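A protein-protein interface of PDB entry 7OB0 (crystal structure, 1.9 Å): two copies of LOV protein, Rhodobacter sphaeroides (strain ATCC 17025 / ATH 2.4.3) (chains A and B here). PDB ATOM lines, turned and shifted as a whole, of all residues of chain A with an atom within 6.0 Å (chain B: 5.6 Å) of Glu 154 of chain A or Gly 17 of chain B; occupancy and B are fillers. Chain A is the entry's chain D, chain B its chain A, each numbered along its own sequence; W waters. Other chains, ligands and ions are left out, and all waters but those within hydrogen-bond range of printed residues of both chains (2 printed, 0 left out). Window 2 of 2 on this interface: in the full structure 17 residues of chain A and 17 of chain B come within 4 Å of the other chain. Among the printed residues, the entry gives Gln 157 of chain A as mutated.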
ATOM      1  N   GLY A 137      23.040   1.096  25.539  1.00  0.00           N
ATOM      2  CA  GLY A 137      21.988   2.049  25.878  1.00  0.00           C
ATOM      3  C   GLY A 137      21.451   2.791  24.667  1.00  0.00           C
ATOM      4  O   GLY A 137      20.240   3.000  24.540  1.00  0.00           O
ATOM      5  N   THR A 140      19.305   0.283  22.843  1.00  0.00           N
ATOM      6  CA  THR A 140      17.997   0.069  23.451  1.00  0.00           C
ATOM      7  C   THR A 140      17.035   1.189  23.068  1.00  0.00           C
ATOM      8  O   THR A 140      15.860   0.936  22.784  1.00  0.00           O
ATOM      9  CB  THR A 140      18.145  -0.070  24.968  1.00  0.00           C
ATOM     10  OG1 THR A 140      19.023  -1.174  25.233  1.00  0.00           O
ATOM     11  CG2 THR A 140      16.810  -0.368  25.596  1.00  0.00           C
ATOM     12  N   GLY A 141      17.531   2.426  22.997  1.00  0.00           N
ATOM     13  CA  GLY A 141      16.690   3.512  22.517  1.00  0.00           C
ATOM     14  C   GLY A 141      16.144   3.257  21.124  1.00  0.00           C
ATOM     15  O   GLY A 141      14.978   3.547  20.841  1.00  0.00           O
ATOM     16  N   GLU A 142      16.978   2.709  20.231  1.00  0.00           N
ATOM     17  CA  GLU A 142      16.505   2.397  18.883  1.00  0.00           C
ATOM     18  C   GLU A 142      15.494   1.259  18.898  1.00  0.00           C
ATOM     19  O   GLU A 142      14.494   1.298  18.171  1.00  0.00           O
ATOM     20  CB  GLU A 142      17.676   2.045  17.961  1.00  0.00           C
ATOM     21  CG  GLU A 142      18.824   3.036  17.940  1.00  0.00           C
ATOM     22  CD  GLU A 142      18.438   4.437  17.461  1.00  0.00           C
ATOM     23  OE1 GLU A 142      17.250   4.724  17.230  1.00  0.00           O
ATOM     24  OE2 GLU A 142      19.349   5.263  17.323  1.00  0.00           O
ATOM     25  N   ALA A 144      13.428   0.623  21.262  1.00  0.00           N
ATOM     26  CA  ALA A 144      12.175   1.212  21.724  1.00  0.00           C
ATOM     27  C   ALA A 144      11.504   2.001  20.611  1.00  0.00           C
ATOM     28  O   ALA A 144      10.275   1.984  20.480  1.00  0.00           O
ATOM     29  CB  ALA A 144      12.430   2.105  22.938  1.00  0.00           C
ATOM     30  N   VAL A 149      11.023  -3.069  21.897  1.00  0.00           N
ATOM     31  CA  VAL A 149      11.039  -2.979  23.351  1.00  0.00           C
ATOM     32  C   VAL A 149       9.990  -1.958  23.766  1.00  0.00           C
ATOM     33  O   VAL A 149      10.007  -0.809  23.301  1.00  0.00           O
ATOM     34  CB  VAL A 149      12.432  -2.618  23.890  1.00  0.00           C
ATOM     35  CG1 VAL A 149      12.389  -2.514  25.417  1.00  0.00           C
ATOM     36  CG2 VAL A 149      13.459  -3.682  23.447  1.00  0.00           C
ATOM     37  N   ALA A 150       9.070  -2.387  24.629  1.00  0.00           N
ATOM     38  CA  ALA A 150       7.967  -1.542  25.064  1.00  0.00           C
ATOM     39  C   ALA A 150       8.469  -0.400  25.936  1.00  0.00           C
ATOM     40  O   ALA A 150       9.463  -0.530  26.658  1.00  0.00           O
ATOM     41  CB  ALA A 150       6.934  -2.365  25.834  1.00  0.00           C
ATOM     42  N   ALA A 151       7.751   0.726  25.871  1.00  0.00           N
ATOM     43  CA  ALA A 151       8.181   1.932  26.573  1.00  0.00           C
ATOM     44  C   ALA A 151       8.379   1.667  28.059  1.00  0.00           C
ATOM     45  O   ALA A 151       9.426   2.004  28.623  1.00  0.00           O
ATOM     46  CB  ALA A 151       7.165   3.053  26.354  1.00  0.00           C
ATOM     47  N   ARG A 152       7.383   1.049  28.710  1.00  0.00           N
ATOM     48  CA  ARG A 152       7.483   0.743  30.135  1.00  0.00           C
ATOM     49  C   ARG A 152       8.648  -0.189  30.457  1.00  0.00           C
ATOM     50  O   ARG A 152       9.053  -0.279  31.620  1.00  0.00           O
ATOM     51  CB  ARG A 152       6.175   0.119  30.637  1.00  0.00           C
ATOM     52  N   LEU A 153       9.198  -0.883  29.466  1.00  0.00           N
ATOM     53  CA  LEU A 153      10.270  -1.831  29.713  1.00  0.00           C
ATOM     54  C   LEU A 153      11.637  -1.351  29.249  1.00  0.00           C
ATOM     55  O   LEU A 153      12.613  -2.097  29.393  1.00  0.00           O
ATOM     56  CB  LEU A 153       9.956  -3.178  29.051  1.00  0.00           C
ATOM     57  CG  LEU A 153       8.612  -3.764  29.491  1.00  0.00           C
ATOM     58  CD1 LEU A 153       8.140  -4.839  28.524  1.00  0.00           C
ATOM     59  CD2 LEU A 153       8.702  -4.267  30.927  1.00  0.00           C
ATOM     60  N   GLU A 154      11.743  -0.136  28.704  1.00  0.00           N
ATOM     61  CA  GLU A 154      13.017   0.279  28.115  1.00  0.00           C
ATOM     62  C   GLU A 154      14.118   0.380  29.172  1.00  0.00           C
ATOM     63  O   GLU A 154      15.260  -0.041  28.937  1.00  0.00           O
ATOM     64  CB  GLU A 154      12.853   1.607  27.372  1.00  0.00           C
ATOM     65  CG  GLU A 154      14.070   1.967  26.527  1.00  0.00           C
ATOM     66  CD  GLU A 154      13.971   3.345  25.896  1.00  0.00           C
ATOM     67  OE1 GLU A 154      12.848   3.872  25.773  1.00  0.00           O
ATOM     68  OE2 GLU A 154      15.021   3.900  25.526  1.00  0.00           O
ATOM     69  N   MET A 155      13.799   0.911  30.353  1.00  0.00           N
ATOM     70  CA  MET A 155      14.844   1.074  31.361  1.00  0.00           C
ATOM     71  C   MET A 155      15.385  -0.275  31.838  1.00  0.00           C
ATOM     72  O   MET A 155      16.593  -0.423  32.038  1.00  0.00           O
ATOM     73  CB  MET A 155      14.335   1.919  32.533  1.00  0.00           C
ATOM     74  CG  MET A 155      15.350   2.057  33.654  1.00  0.00           C
ATOM     75  SD  MET A 155      14.649   2.610  35.219  1.00  0.00           S
ATOM     76  CE  MET A 155      14.583   4.362  34.909  1.00  0.00           C
ATOM     77  N   ASP A 156      14.515  -1.271  32.026  1.00  0.00           N
ATOM     78  CA  ASP A 156      15.006  -2.602  32.380  1.00  0.00           C
ATOM     79  C   ASP A 156      15.882  -3.176  31.269  1.00  0.00           C
ATOM     80  O   ASP A 156      16.952  -3.735  31.529  1.00  0.00           O
ATOM     81  CB  ASP A 156      13.845  -3.552  32.663  1.00  0.00           C
ATOM     82  CG  ASP A 156      13.119  -3.244  33.969  1.00  0.00           C
ATOM     83  OD1 ASP A 156      13.722  -2.642  34.879  1.00  0.00           O
ATOM     84  OD2 ASP A 156      11.957  -3.671  34.086  1.00  0.00           O
ATOM     85  N   GLN A 157      15.418  -3.087  30.022  1.00  0.00           N
ATOM     86  CA  GLN A 157      16.206  -3.629  28.918  1.00  0.00           C
ATOM     87  C   GLN A 157      17.541  -2.906  28.787  1.00  0.00           C
ATOM     88  O   GLN A 157      18.562  -3.520  28.465  1.00  0.00           O
ATOM     89  CB  GLN A 157      15.409  -3.550  27.618  1.00  0.00           C
ATOM     90  CG  GLN A 157      16.136  -4.155  26.421  1.00  0.00           C
ATOM     91  CD  GLN A 157      16.267  -5.676  26.504  1.00  0.00           C
ATOM     92  OE1 GLN A 157      15.912  -6.302  27.514  1.00  0.00           O
ATOM     93  NE2 GLN A 157      16.798  -6.276  25.443  1.00  0.00           N
ATOM     94  N   ARG A 158      17.557  -1.596  29.026  1.00  0.00           N
ATOM     95  CA  ARG A 158      18.816  -0.859  28.960  1.00  0.00           C
ATOM     96  C   ARG A 158      19.793  -1.338  30.031  1.00  0.00           C
ATOM     97  O   ARG A 158      20.980  -1.572  29.756  1.00  0.00           O
ATOM     98  CB  ARG A 158      18.532   0.637  29.091  1.00  0.00           C
ATOM     99  CG  ARG A 158      19.762   1.511  29.052  1.00  0.00           C
ATOM    100  CD  ARG A 158      19.379   2.972  28.845  1.00  0.00           C
ATOM    101  NE  ARG A 158      18.630   3.502  29.979  1.00  0.00           N
ATOM    102  CZ  ARG A 158      17.362   3.891  29.907  1.00  0.00           C
ATOM    103  NH1 ARG A 158      16.683   3.809  28.780  1.00  0.00           N
ATOM    104  NH2 ARG A 158      16.767   4.382  30.992  1.00  0.00           N
ATOM    105  N   ARG A 159      19.308  -1.489  31.267  1.00  0.00           N
ATOM    106  CA  ARG A 159      20.136  -2.041  32.336  1.00  0.00           C
ATOM    107  C   ARG A 159      20.681  -3.406  31.955  1.00  0.00           C
ATOM    108  O   ARG A 159      21.880  -3.675  32.100  1.00  0.00           O
ATOM    109  CB  ARG A 159      19.312  -2.152  33.630  1.00  0.00           C
ATOM    110  CG  ARG A 159      20.054  -2.740  34.810  1.00  0.00           C
ATOM    111  CD  ARG A 159      19.083  -3.031  35.962  1.00  0.00           C
ATOM    112  NE  ARG A 159      18.189  -4.133  35.617  1.00  0.00           N
ATOM    113  CZ  ARG A 159      16.870  -4.042  35.520  1.00  0.00           C
ATOM    114  NH1 ARG A 159      16.226  -2.930  35.830  1.00  0.00           N
ATOM    115  NH2 ARG A 159      16.174  -5.101  35.116  1.00  0.00           N
ATOM    116  N   ARG B  15       8.928  11.715  23.920  1.00  0.00           N
ATOM    117  CA  ARG B  15       8.990  10.289  23.649  1.00  0.00           C
ATOM    118  C   ARG B  15      10.279   9.638  24.133  1.00  0.00           C
ATOM    119  O   ARG B  15      10.449   8.430  23.964  1.00  0.00           O
ATOM    120  CB  ARG B  15       8.750  10.034  22.152  1.00  0.00           C
ATOM    121  CG  ARG B  15       9.852  10.426  21.204  1.00  0.00           C
ATOM    122  CD  ARG B  15       9.540   9.900  19.806  1.00  0.00           C
ATOM    123  N   SER B  16      11.158  10.382  24.792  1.00  0.00           N
ATOM    124  CA  SER B  16      12.409   9.795  25.257  1.00  0.00           C
ATOM    125  C   SER B  16      12.187   8.813  26.398  1.00  0.00           C
ATOM    126  O   SER B  16      11.347   9.028  27.273  1.00  0.00           O
ATOM    127  CB  SER B  16      13.369  10.879  25.727  1.00  0.00           C
ATOM    128  OG  SER B  16      14.610  10.283  26.081  1.00  0.00           O
ATOM    129  N   GLY B  17      12.988   7.750  26.407  1.00  0.00           N
ATOM    130  CA  GLY B  17      13.041   6.843  27.538  1.00  0.00           C
ATOM    131  C   GLY B  17      13.962   7.249  28.672  1.00  0.00           C
ATOM    132  O   GLY B  17      14.038   6.541  29.682  1.00  0.00           O
ATOM    133  N   VAL B  18      14.679   8.362  28.562  1.00  0.00           N
ATOM    134  CA  VAL B  18      15.482   8.857  29.674  1.00  0.00           C
ATOM    135  C   VAL B  18      14.876  10.170  30.174  1.00  0.00           C
ATOM    136  O   VAL B  18      14.248  10.920  29.419  1.00  0.00           O
ATOM    137  CB  VAL B  18      16.973   9.040  29.303  1.00  0.00           C
ATOM    138  CG1 VAL B  18      17.645   7.687  29.054  1.00  0.00           C
ATOM    139  CG2 VAL B  18      17.137   9.975  28.084  1.00  0.00           C
ATOM    140  N   ALA B  19      15.040  10.424  31.474  1.00  0.00           N
ATOM    141  CA  ALA B  19      14.649  11.705  32.050  1.00  0.00           C
ATOM    142  C   ALA B  19      15.392  12.866  31.388  1.00  0.00           C
ATOM    143  O   ALA B  19      16.624  12.848  31.250  1.00  0.00           O
ATOM    144  CB  ALA B  19      14.912  11.702  33.563  1.00  0.00           C
ATOM    145  N   PRO B  38       9.585  10.570  32.091  1.00  0.00           N
ATOM    146  CA  PRO B  38      10.522   9.879  32.994  1.00  0.00           C
ATOM    147  C   PRO B  38      11.018  10.767  34.118  1.00  0.00           C
ATOM    148  O   PRO B  38      11.207  10.286  35.240  1.00  0.00           O
ATOM    149  CB  PRO B  38      11.665   9.452  32.064  1.00  0.00           C
ATOM    150  CG  PRO B  38      11.020   9.300  30.750  1.00  0.00           C
ATOM    151  CD  PRO B  38       9.997  10.394  30.682  1.00  0.00           C
ATOM    152  N   ARG B  41       8.161  11.018  36.670  1.00  0.00           N
ATOM    153  CA  ARG B  41       7.985   9.779  37.425  1.00  0.00           C
ATOM    154  C   ARG B  41       9.054   9.628  38.497  1.00  0.00           C
ATOM    155  O   ARG B  41       8.777   9.150  39.608  1.00  0.00           O
ATOM    156  CB  ARG B  41       8.012   8.570  36.490  1.00  0.00           C
ATOM    157  CG  ARG B  41       6.734   8.381  35.690  1.00  0.00           C
ATOM    158  CD  ARG B  41       6.676   6.998  35.049  1.00  0.00           C
ATOM    159  NE  ARG B  41       7.946   6.591  34.460  1.00  0.00           N
ATOM    160  CZ  ARG B  41       8.325   6.835  33.210  1.00  0.00           C
ATOM    161  NH1 ARG B  41       7.546   7.491  32.361  1.00  0.00           N
ATOM    162  NH2 ARG B  41       9.516   6.402  32.799  1.00  0.00           N
ATOM    163  N   ALA B 138      22.108   6.265  25.791  1.00  0.00           N
ATOM    164  CA  ALA B 138      20.764   6.669  25.378  1.00  0.00           C
ATOM    165  C   ALA B 138      20.648   8.186  25.304  1.00  0.00           C
ATOM    166  O   ALA B 138      20.051   8.730  24.369  1.00  0.00           O
ATOM    167  CB  ALA B 138      19.725   6.127  26.363  1.00  0.00           C
ATOM    168  N   GLU B 142      19.785  11.075  22.193  1.00  0.00           N
ATOM    169  CA  GLU B 142      18.832  12.189  22.229  1.00  0.00           C
ATOM    170  C   GLU B 142      19.513  13.517  21.913  1.00  0.00           C
ATOM    171  O   GLU B 142      18.931  14.365  21.224  1.00  0.00           O
ATOM    172  CB  GLU B 142      18.124  12.251  23.590  1.00  0.00           C
ATOM    173  CG  GLU B 142      17.443  10.931  24.042  1.00  0.00           C
ATOM    174  CD  GLU B 142      16.266  10.498  23.164  1.00  0.00           C
ATOM    175  OE1 GLU B 142      16.199  10.858  21.956  1.00  0.00           O
ATOM    176  OE2 GLU B 142      15.415   9.750  23.681  1.00  0.00           O
HETATM  177  O   HOH W   1      14.181   6.026  32.211  1.00  0.00           O
HETATM  178  O   HOH W   2      13.681   4.099  29.651  1.00  0.00           O
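Water W2 lies within hydrogen-bond range of O of Gly 17 of chain B (2.5 Å), NH1 of Arg 158 of chain A (3.1 Å) and N of Met 155 of chain A (3.3 Å). Water W1 bridges the backbone carbonyl oxygen (O) of Gly 17 of chain B (2.6 Å) and the guanidinium group (NH2) of Arg 158 of chain A (3.3 Å).
Ala 138 of chain B touches Gly 137 of chain A (CB to O, 3.7 Å). OE1 of Glu 154 of chain A touches CA of Gly 17 of chain B (3.5 Å). O of Gly 17 of chain B touches NH2 of Arg 158 of chain A (3.7 Å). Val 18 of chain B touches Arg 158 of chain A.
Among the printed residues, 4 pairs touch across the chains. Among the printed residues, no Asp or Glu carboxylate lies within 4 Å of a Lys or Arg side-chain nitrogen of the other chain.
OG of Ser 16 of chain B is in hydrogen-bond range of N of Val 18 of chain B (3.1 Å). The side-chain carboxylate (OE2) of Glu 154 of chain A lies within salt-bridge range of the guanidinium group (NH1) of Arg 158 of chain A.
Position printed for both chains: 142. Of the 4 pairs that touch across the chains among the printed residues, none has its exchanged pair printed and touching as well.
Of chain B, only Gly 17 (3.5 Å) comes within 4 Å of Glu 154 of chain A. Gly 17 of chain B touches just these residues of chain A: Glu 154 (3.5 Å) and Arg 158 (3.7 Å). Printed residues of chain A within 4 Å of Ala 138 of chain B: Gly 137. Printed residues of chain B within 4 Å of Arg 158 of chain A: Gly 17 (3.7 Å) and Val 18 (3.9 Å). Printed residues of chain B within 4 Å of Gly 137 of chain A: Ala 138 (3.7 Å). Of the printed residues of chain A, Val 18 of chain B touches Arg 158 (3.9 Å). Ala 19 of chain B touches none of the printed residues of chain A. The nearest printed residue of chain B that does not touch Gly 137 of chain A is Val 18 of chain B (7.0 Å).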
